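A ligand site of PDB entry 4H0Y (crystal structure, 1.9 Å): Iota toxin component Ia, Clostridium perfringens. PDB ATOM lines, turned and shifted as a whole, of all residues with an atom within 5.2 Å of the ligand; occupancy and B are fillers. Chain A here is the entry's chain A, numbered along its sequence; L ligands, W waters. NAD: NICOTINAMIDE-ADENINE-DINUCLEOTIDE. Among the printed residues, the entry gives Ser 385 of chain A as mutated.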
ATOM      1  N   TYR A 256      11.335  22.090  28.836  1.00  0.00           N
ATOM      2  CA  TYR A 256      12.740  21.714  28.636  1.00  0.00           C
ATOM      3  C   TYR A 256      13.709  22.844  28.901  1.00  0.00           C
ATOM      4  O   TYR A 256      14.782  22.616  29.462  1.00  0.00           O
ATOM      5  CB  TYR A 256      12.996  21.076  27.251  1.00  0.00           C
ATOM      6  CG  TYR A 256      12.793  21.940  26.010  1.00  0.00           C
ATOM      7  CD1 TYR A 256      11.657  21.793  25.218  1.00  0.00           C
ATOM      8  CD2 TYR A 256      13.777  22.835  25.578  1.00  0.00           C
ATOM      9  CE1 TYR A 256      11.477  22.534  24.065  1.00  0.00           C
ATOM     10  CE2 TYR A 256      13.597  23.589  24.428  1.00  0.00           C
ATOM     11  CZ  TYR A 256      12.454  23.437  23.676  1.00  0.00           C
ATOM     12  OH  TYR A 256      12.277  24.183  22.531  1.00  0.00           O
ATOM     13  N   ASN A 260      16.406  22.139  31.577  1.00  0.00           N
ATOM     14  CA  ASN A 260      17.765  22.004  31.051  1.00  0.00           C
ATOM     15  C   ASN A 260      18.713  23.104  31.551  1.00  0.00           C
ATOM     16  O   ASN A 260      19.884  22.821  31.822  1.00  0.00           O
ATOM     17  CB  ASN A 260      17.759  21.940  29.516  1.00  0.00           C
ATOM     18  CG  ASN A 260      17.239  20.597  28.992  1.00  0.00           C
ATOM     19  OD1 ASN A 260      17.220  19.600  29.718  1.00  0.00           O
ATOM     20  ND2 ASN A 260      16.849  20.571  27.717  1.00  0.00           N
ATOM     21  N   ILE A 264      22.161  22.537  33.426  1.00  0.00           N
ATOM     22  CA  ILE A 264      23.404  23.127  32.920  1.00  0.00           C
ATOM     23  C   ILE A 264      24.050  24.037  33.964  1.00  0.00           C
ATOM     24  O   ILE A 264      25.283  24.081  34.067  1.00  0.00           O
ATOM     25  CB  ILE A 264      23.204  23.892  31.592  1.00  0.00           C
ATOM     26  CG1 ILE A 264      22.856  22.911  30.460  1.00  0.00           C
ATOM     27  CG2 ILE A 264      24.467  24.651  31.208  1.00  0.00           C
ATOM     28  CD1 ILE A 264      22.267  23.564  29.230  1.00  0.00           C
ATOM     29  N   TYR A 299      20.638  12.220  14.452  1.00  0.00           N
ATOM     30  CA  TYR A 299      21.228  13.448  13.924  1.00  0.00           C
ATOM     31  C   TYR A 299      20.746  14.624  14.755  1.00  0.00           C
ATOM     32  O   TYR A 299      19.584  14.671  15.172  1.00  0.00           O
ATOM     33  CB  TYR A 299      20.833  13.629  12.462  1.00  0.00           C
ATOM     34  CG  TYR A 299      21.306  12.510  11.565  1.00  0.00           C
ATOM     35  CD1 TYR A 299      20.602  11.311  11.492  1.00  0.00           C
ATOM     36  CD2 TYR A 299      22.472  12.639  10.822  1.00  0.00           C
ATOM     37  CE1 TYR A 299      21.043  10.275  10.687  1.00  0.00           C
ATOM     38  CE2 TYR A 299      22.923  11.603  10.014  1.00  0.00           C
ATOM     39  CZ  TYR A 299      22.198  10.424   9.947  1.00  0.00           C
ATOM     40  OH  TYR A 299      22.648   9.402   9.143  1.00  0.00           O
ATOM     41  N   ARG A 300      21.637  15.572  15.003  1.00  0.00           N
ATOM     42  CA  ARG A 300      21.283  16.800  15.699  1.00  0.00           C
ATOM     43  C   ARG A 300      21.969  17.959  15.020  1.00  0.00           C
ATOM     44  O   ARG A 300      23.169  17.917  14.778  1.00  0.00           O
ATOM     45  CB  ARG A 300      21.688  16.743  17.172  1.00  0.00           C
ATOM     46  CG  ARG A 300      21.690  18.097  17.865  1.00  0.00           C
ATOM     47  CD  ARG A 300      21.963  18.005  19.345  1.00  0.00           C
ATOM     48  NE  ARG A 300      21.876  19.343  19.895  1.00  0.00           N
ATOM     49  CZ  ARG A 300      20.742  19.957  20.230  1.00  0.00           C
ATOM     50  NH1 ARG A 300      19.561  19.342  20.130  1.00  0.00           N
ATOM     51  NH2 ARG A 300      20.792  21.209  20.685  1.00  0.00           N
ATOM     52  N   ARG A 301      21.185  18.976  14.722  1.00  0.00           N
ATOM     53  CA  ARG A 301      21.740  20.223  14.253  1.00  0.00           C
ATOM     54  C   ARG A 301      21.996  21.119  15.458  1.00  0.00           C
ATOM     55  O   ARG A 301      21.071  21.688  16.045  1.00  0.00           O
ATOM     56  CB  ARG A 301      20.790  20.847  13.231  1.00  0.00           C
ATOM     57  CG  ARG A 301      21.199  20.540  11.794  1.00  0.00           C
ATOM     58  CD  ARG A 301      20.459  19.519  10.933  1.00  0.00           C
ATOM     59  NE  ARG A 301      20.843  20.129   9.666  1.00  0.00           N
ATOM     60  CZ  ARG A 301      21.049  19.647   8.442  1.00  0.00           C
ATOM     61  NH1 ARG A 301      20.789  18.395   7.996  1.00  0.00           N
ATOM     62  NH2 ARG A 301      21.489  20.575   7.582  1.00  0.00           N
ATOM     63  N   SER A 302      23.280  21.216  15.824  1.00  0.00           N
ATOM     64  CA  SER A 302      23.707  21.932  17.027  1.00  0.00           C
ATOM     65  C   SER A 302      23.741  23.423  16.807  1.00  0.00           C
ATOM     66  O   SER A 302      24.122  23.893  15.727  1.00  0.00           O
ATOM     67  CB  SER A 302      25.096  21.456  17.456  1.00  0.00           C
ATOM     68  OG  SER A 302      25.045  20.143  18.004  1.00  0.00           O
ATOM     69  N   GLY A 303      23.371  24.176  17.837  1.00  0.00           N
ATOM     70  CA  GLY A 303      23.671  25.594  17.870  1.00  0.00           C
ATOM     71  C   GLY A 303      25.158  25.762  18.142  1.00  0.00           C
ATOM     72  O   GLY A 303      25.777  24.900  18.761  1.00  0.00           O
ATOM     73  N   PRO A 304      25.742  26.881  17.677  1.00  0.00           N
ATOM     74  CA  PRO A 304      27.177  27.050  17.891  1.00  0.00           C
ATOM     75  C   PRO A 304      27.585  27.133  19.365  1.00  0.00           C
ATOM     76  O   PRO A 304      28.765  26.923  19.686  1.00  0.00           O
ATOM     77  CB  PRO A 304      27.498  28.370  17.170  1.00  0.00           C
ATOM     78  CG  PRO A 304      26.194  29.055  17.002  1.00  0.00           C
ATOM     79  CD  PRO A 304      25.179  27.966  16.868  1.00  0.00           C
ATOM     80  N   GLN A 305      26.632  27.406  20.258  1.00  0.00           N
ATOM     81  CA  GLN A 305      26.954  27.595  21.672  1.00  0.00           C
ATOM     82  C   GLN A 305      27.351  26.281  22.349  1.00  0.00           C
ATOM     83  O   GLN A 305      28.066  26.293  23.354  1.00  0.00           O
ATOM     84  CB  GLN A 305      25.813  28.272  22.445  1.00  0.00           C
ATOM     85  CG  GLN A 305      25.508  29.693  21.955  1.00  0.00           C
ATOM     86  CD  GLN A 305      24.531  29.773  20.778  1.00  0.00           C
ATOM     87  OE1 GLN A 305      24.252  30.877  20.307  1.00  0.00           O
ATOM     88  NE2 GLN A 305      23.995  28.639  20.315  1.00  0.00           N
ATOM     89  N   GLU A 306      26.890  25.162  21.799  1.00  0.00           N
ATOM     90  CA  GLU A 306      27.317  23.842  22.282  1.00  0.00           C
ATOM     91  C   GLU A 306      28.812  23.581  22.074  1.00  0.00           C
ATOM     92  O   GLU A 306      29.405  22.739  22.749  1.00  0.00           O
ATOM     93  CB  GLU A 306      26.503  22.754  21.585  1.00  0.00           C
ATOM     94  CG  GLU A 306      25.061  22.702  22.015  1.00  0.00           C
ATOM     95  CD  GLU A 306      24.168  22.068  20.975  1.00  0.00           C
ATOM     96  OE1 GLU A 306      24.364  20.870  20.670  1.00  0.00           O
ATOM     97  OE2 GLU A 306      23.265  22.758  20.459  1.00  0.00           O
ATOM     98  N   THR A 337      30.177  16.364  26.976  1.00  0.00           N
ATOM     99  CA  THR A 337      29.095  15.949  27.860  1.00  0.00           C
ATOM    100  C   THR A 337      28.030  17.040  27.951  1.00  0.00           C
ATOM    101  O   THR A 337      28.349  18.240  28.021  1.00  0.00           O
ATOM    102  CB  THR A 337      29.631  15.530  29.242  1.00  0.00           C
ATOM    103  OG1 THR A 337      28.555  15.048  30.056  1.00  0.00           O
ATOM    104  CG2 THR A 337      30.312  16.673  29.944  1.00  0.00           C
ATOM    105  N   TYR A 338      26.771  16.605  27.936  1.00  0.00           N
ATOM    106  CA  TYR A 338      25.609  17.485  28.008  1.00  0.00           C
ATOM    107  C   TYR A 338      24.951  17.252  29.359  1.00  0.00           C
ATOM    108  O   TYR A 338      24.397  16.185  29.585  1.00  0.00           O
ATOM    109  CB  TYR A 338      24.620  17.140  26.888  1.00  0.00           C
ATOM    110  CG  TYR A 338      25.003  17.681  25.530  1.00  0.00           C
ATOM    111  CD1 TYR A 338      24.367  18.794  24.985  1.00  0.00           C
ATOM    112  CD2 TYR A 338      26.006  17.068  24.782  1.00  0.00           C
ATOM    113  CE1 TYR A 338      24.720  19.291  23.744  1.00  0.00           C
ATOM    114  CE2 TYR A 338      26.369  17.553  23.532  1.00  0.00           C
ATOM    115  CZ  TYR A 338      25.721  18.664  23.015  1.00  0.00           C
ATOM    116  OH  TYR A 338      26.080  19.144  21.782  1.00  0.00           O
ATOM    117  N   PRO A 339      25.018  18.245  30.265  1.00  0.00           N
ATOM    118  CA  PRO A 339      24.284  18.024  31.523  1.00  0.00           C
ATOM    119  C   PRO A 339      22.768  17.993  31.311  1.00  0.00           C
ATOM    120  O   PRO A 339      22.044  17.330  32.062  1.00  0.00           O
ATOM    121  CB  PRO A 339      24.672  19.230  32.386  1.00  0.00           C
ATOM    122  CG  PRO A 339      25.811  19.896  31.699  1.00  0.00           C
ATOM    123  CD  PRO A 339      25.770  19.508  30.252  1.00  0.00           C
ATOM    124  N   ASN A 340      22.309  18.707  30.295  1.00  0.00           N
ATOM    125  CA  ASN A 340      20.903  18.717  29.890  1.00  0.00           C
ATOM    126  C   ASN A 340      20.458  17.441  29.176  1.00  0.00           C
ATOM    127  O   ASN A 340      21.278  16.697  28.622  1.00  0.00           O
ATOM    128  CB  ASN A 340      20.591  19.924  28.990  1.00  0.00           C
ATOM    129  CG  ASN A 340      21.606  20.145  27.869  1.00  0.00           C
ATOM    130  OD1 ASN A 340      22.820  19.984  28.059  1.00  0.00           O
ATOM    131  ND2 ASN A 340      21.114  20.530  26.695  1.00  0.00           N
ATOM    132  N   SER A 343      17.939  16.595  22.524  1.00  0.00           N
ATOM    133  CA  SER A 343      17.078  16.077  21.467  1.00  0.00           C
ATOM    134  C   SER A 343      17.862  15.826  20.181  1.00  0.00           C
ATOM    135  O   SER A 343      18.788  16.574  19.836  1.00  0.00           O
ATOM    136  CB  SER A 343      15.935  17.044  21.189  1.00  0.00           C
ATOM    137  OG  SER A 343      16.428  18.310  20.796  1.00  0.00           O
ATOM    138  N   THR A 344      17.462  14.773  19.494  1.00  0.00           N
ATOM    139  CA  THR A 344      18.047  14.366  18.220  1.00  0.00           C
ATOM    140  C   THR A 344      16.927  13.883  17.320  1.00  0.00           C
ATOM    141  O   THR A 344      15.796  13.704  17.775  1.00  0.00           O
ATOM    142  CB  THR A 344      19.043  13.204  18.401  1.00  0.00           C
ATOM    143  OG1 THR A 344      18.341  12.020  18.804  1.00  0.00           O
ATOM    144  CG2 THR A 344      20.089  13.538  19.465  1.00  0.00           C
ATOM    145  N   SER A 345      17.234  13.662  16.051  1.00  0.00           N
ATOM    146  CA  SER A 345      16.261  13.139  15.098  1.00  0.00           C
ATOM    147  C   SER A 345      16.725  11.840  14.449  1.00  0.00           C
ATOM    148  O   SER A 345      17.933  11.655  14.240  1.00  0.00           O
ATOM    149  CB  SER A 345      15.991  14.171  14.004  1.00  0.00           C
ATOM    150  OG  SER A 345      15.036  13.704  13.062  1.00  0.00           O
ATOM    151  N   PHE A 354      16.084  24.852  11.628  1.00  0.00           N
ATOM    152  CA  PHE A 354      17.536  24.933  11.793  1.00  0.00           C
ATOM    153  C   PHE A 354      18.289  24.909  10.469  1.00  0.00           C
ATOM    154  O   PHE A 354      19.416  24.398  10.373  1.00  0.00           O
ATOM    155  CB  PHE A 354      18.061  23.862  12.747  1.00  0.00           C
ATOM    156  CG  PHE A 354      17.540  22.488  12.488  1.00  0.00           C
ATOM    157  CD1 PHE A 354      17.738  21.834  11.270  1.00  0.00           C
ATOM    158  CD2 PHE A 354      16.911  21.802  13.510  1.00  0.00           C
ATOM    159  CE1 PHE A 354      17.269  20.552  11.075  1.00  0.00           C
ATOM    160  CE2 PHE A 354      16.447  20.516  13.327  1.00  0.00           C
ATOM    161  CZ  PHE A 354      16.631  19.892  12.109  1.00  0.00           C
ATOM    162  N   ARG A 357      21.977  26.226  10.661  1.00  0.00           N
ATOM    163  CA  ARG A 357      22.930  25.665  11.622  1.00  0.00           C
ATOM    164  C   ARG A 357      24.045  24.912  10.899  1.00  0.00           C
ATOM    165  O   ARG A 357      23.773  24.136   9.973  1.00  0.00           O
ATOM    166  CB  ARG A 357      22.229  24.753  12.627  1.00  0.00           C
ATOM    167  CG  ARG A 357      21.489  25.550  13.685  1.00  0.00           C
ATOM    168  CD  ARG A 357      20.946  24.663  14.786  1.00  0.00           C
ATOM    169  NE  ARG A 357      20.357  25.460  15.850  1.00  0.00           N
ATOM    170  CZ  ARG A 357      19.770  24.983  16.943  1.00  0.00           C
ATOM    171  NH1 ARG A 357      19.680  23.669  17.160  1.00  0.00           N
ATOM    172  NH2 ARG A 357      19.260  25.817  17.846  1.00  0.00           N
ATOM    173  N   GLU A 383       9.039  16.311  14.106  1.00  0.00           N
ATOM    174  CA  GLU A 383      10.477  16.359  14.376  1.00  0.00           C
ATOM    175  C   GLU A 383      11.179  15.006  14.248  1.00  0.00           C
ATOM    176  O   GLU A 383      12.410  14.950  14.125  1.00  0.00           O
ATOM    177  CB  GLU A 383      10.728  16.954  15.766  1.00  0.00           C
ATOM    178  CG  GLU A 383       9.703  16.547  16.819  1.00  0.00           C
ATOM    179  CD  GLU A 383       9.543  17.602  17.892  1.00  0.00           C
ATOM    180  OE1 GLU A 383       8.473  18.250  17.930  1.00  0.00           O
ATOM    181  OE2 GLU A 383      10.475  17.786  18.695  1.00  0.00           O
ATOM    182  N   SER A 385      11.620  12.764  16.577  1.00  0.00           N
ATOM    183  CA  SER A 385      12.584  13.034  17.629  1.00  0.00           C
ATOM    184  C   SER A 385      12.883  11.848  18.531  1.00  0.00           C
ATOM    185  O   SER A 385      11.986  11.081  18.892  1.00  0.00           O
ATOM    186  CB  SER A 385      12.117  14.198  18.498  1.00  0.00           C
ATOM    187  OG  SER A 385      12.320  15.431  17.836  1.00  0.00           O
HETATM  188  PA  NAD L   1      18.137  23.234  22.695  1.00  0.00           P
HETATM  189  O1A NAD L   1      17.175  23.434  23.846  1.00  0.00           O
HETATM  190  O2A NAD L   1      18.855  21.923  22.504  1.00  0.00           O
HETATM  191  O5B NAD L   1      19.244  24.403  22.723  1.00  0.00           O
HETATM  192  C5B NAD L   1      18.920  25.760  23.054  1.00  0.00           C
HETATM  193  C4B NAD L   1      20.201  26.594  23.001  1.00  0.00           C
HETATM  194  O4B NAD L   1      21.103  26.144  24.008  1.00  0.00           O
HETATM  195  C3B NAD L   1      20.952  26.448  21.688  1.00  0.00           C
HETATM  196  O3B NAD L   1      21.659  27.664  21.372  1.00  0.00           O
HETATM  197  C2B NAD L   1      21.938  25.321  21.946  1.00  0.00           C
HETATM  198  O2B NAD L   1      23.098  25.412  21.108  1.00  0.00           O
HETATM  199  C1B NAD L   1      22.291  25.604  23.392  1.00  0.00           C
HETATM  200  N9A NAD L   1      22.704  24.441  24.203  1.00  0.00           N
HETATM  201  C8A NAD L   1      22.012  23.317  24.439  1.00  0.00           C
HETATM  202  N7A NAD L   1      22.716  22.498  25.260  1.00  0.00           N
HETATM  203  C5A NAD L   1      23.861  23.126  25.573  1.00  0.00           C
HETATM  204  C6A NAD L   1      25.044  22.819  26.398  1.00  0.00           C
HETATM  205  N6A NAD L   1      25.114  21.635  27.066  1.00  0.00           N
HETATM  206  N1A NAD L   1      26.031  23.748  26.454  1.00  0.00           N
HETATM  207  C2A NAD L   1      25.965  24.923  25.790  1.00  0.00           C
HETATM  208  N3A NAD L   1      24.904  25.259  25.022  1.00  0.00           N
HETATM  209  C4A NAD L   1      23.855  24.409  24.880  1.00  0.00           C
HETATM  210  O3  NAD L   1      17.373  23.683  21.345  1.00  0.00           O
HETATM  211  PN  NAD L   1      17.155  22.778  20.028  1.00  0.00           P
HETATM  212  O1N NAD L   1      17.563  21.329  20.283  1.00  0.00           O
HETATM  213  O2N NAD L   1      17.724  23.532  18.830  1.00  0.00           O
HETATM  214  O5D NAD L   1      15.565  22.895  19.906  1.00  0.00           O
HETATM  215  C5D NAD L   1      14.752  22.117  20.758  1.00  0.00           C
HETATM  216  C4D NAD L   1      13.487  21.846  19.977  1.00  0.00           C
HETATM  217  O4D NAD L   1      13.777  21.290  18.691  1.00  0.00           O
HETATM  218  C3D NAD L   1      12.783  20.780  20.763  1.00  0.00           C
HETATM  219  O3D NAD L   1      11.369  20.857  20.545  1.00  0.00           O
HETATM  220  C2D NAD L   1      13.369  19.510  20.170  1.00  0.00           C
HETATM  221  O2D NAD L   1      12.512  18.383  20.358  1.00  0.00           O
HETATM  222  C1D NAD L   1      13.510  19.876  18.694  1.00  0.00           C
HETATM  223  N1N NAD L   1      14.545  19.082  18.004  1.00  0.00           N
HETATM  224  C2N NAD L   1      15.743  19.581  17.644  1.00  0.00           C
HETATM  225  C3N NAD L   1      16.691  18.798  16.983  1.00  0.00           C
HETATM  226  C7N NAD L   1      18.043  19.334  16.561  1.00  0.00           C
HETATM  227  O7N NAD L   1      18.634  18.776  15.655  1.00  0.00           O
HETATM  228  N7N NAD L   1      18.577  20.413  17.150  1.00  0.00           N
HETATM  229  C4N NAD L   1      16.381  17.473  16.675  1.00  0.00           C
HETATM  230  C5N NAD L   1      15.136  16.968  17.051  1.00  0.00           C
HETATM  231  C6N NAD L   1      14.236  17.802  17.717  1.00  0.00           C
HETATM  232  O   HOH W   1      27.758  24.158  28.698  1.00  0.00           O
HETATM  233  O   HOH W   2      16.137  25.804  25.424  1.00  0.00           O
HETATM  234  O   HOH W   3      20.483  20.375  23.892  1.00  0.00           O
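Tyr 256 touches the ligand (CE2 to O1A, 3.6 Å).
Gly 303 touches the ligand (CA to O2B, 3.3 Å).
Tyr 338 touches the ligand.
CD of Pro 339 touches N6A of the ligand, at 3.9 Å.
O of Thr 344 touches C5N of the ligand (3.4 Å).
Ser 345 touches the ligand.
CE2 of Phe 354 touches O7N of the ligand (3.6 Å).
OG of Ser 385 touches C6N of the ligand, at 3.1 Å.
Hydrophobic or aromatic side chains that line the ligand: Tyr 256, Tyr 338, Pro 339 and Phe 354.
Of the 22 residues printed, 16 come within 4 Å of the ligand.
The guanidinium group (NH1) of Arg 357 is in hydrogen-bond range of the backbone carbonyl oxygen (O) of Arg 301 (2.7 Å).
The side-chain carboxylate of Glu 383 lies close to the side-chain hydroxyl of Ser 385, 3.1 Å away.
The backbone carbonyl oxygen of Glu 383 sits at hydrogen-bond distance from the side-chain hydroxyl of Ser 345 (3.1 Å).
The side-chain carboxylate (OE2) of Glu 306 is in salt-bridge range of the guanidinium group (NH2) of Arg 300 (2.9 Å).
The side-chain carboxylate of Glu 306 lies within hydrogen-bond range of the backbone NH of Gly 303 (3.0 Å).
The side-chain carboxylate (OE1) of Glu 306 sits at hydrogen-bond distance from the side-chain hydroxyl (OH) of Tyr 338 (2.7 Å).
The guanidinium group (NH1) of Arg 300 is in hydrogen-bond range of the backbone carbonyl oxygen (O) of Ser 343 (2.9 Å).
The backbone NH (N) of Ser 345 sits at hydrogen-bond distance from the backbone carbonyl oxygen (O) of Tyr 299, 2.7 Å away.
Water W3 lies within hydrogen-bond range of O2A of the ligand (2.6 Å), ND2 of Asn 340 (2.9 Å) and NH2 of Arg 300 (3.3 Å).
The guanidinium group (NH1) of Arg 357 lies within salt-bridge range of an oxygen (O2N) of the ligand, 2.6 Å away.
An oxygen (O2D) of the ligand lies within hydrogen-bond range of the side-chain carboxylate of Glu 383, at 2.7 Å.
The backbone NH (N) of Arg 301 is in hydrogen-bond range of an oxygen (O7N) of the ligand (2.7 Å).
The backbone carbonyl oxygen (O) of Arg 301 sits at hydrogen-bond distance from a nitrogen (N7N) of the ligand, at 3.0 Å.
The side-chain carboxylate (OE2) of Glu 306 is in hydrogen-bond range of an oxygen (O2B) of the ligand.
The side-chain amide nitrogen of Gln 305 lies within hydrogen-bond range of an oxygen (O3B) of the ligand.
An oxygen (O2A) of the ligand is in salt-bridge range of the guanidinium group (NH2) of Arg 300 (2.8 Å).
A nitrogen (N7A) of the ligand is in hydrogen-bond range of the side-chain amide nitrogen (ND2) of Asn 340 (2.9 Å).
An oxygen (O1N) of the ligand sits at hydrogen-bond distance from the side-chain hydroxyl (OG) of Ser 343, 3.3 Å away.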
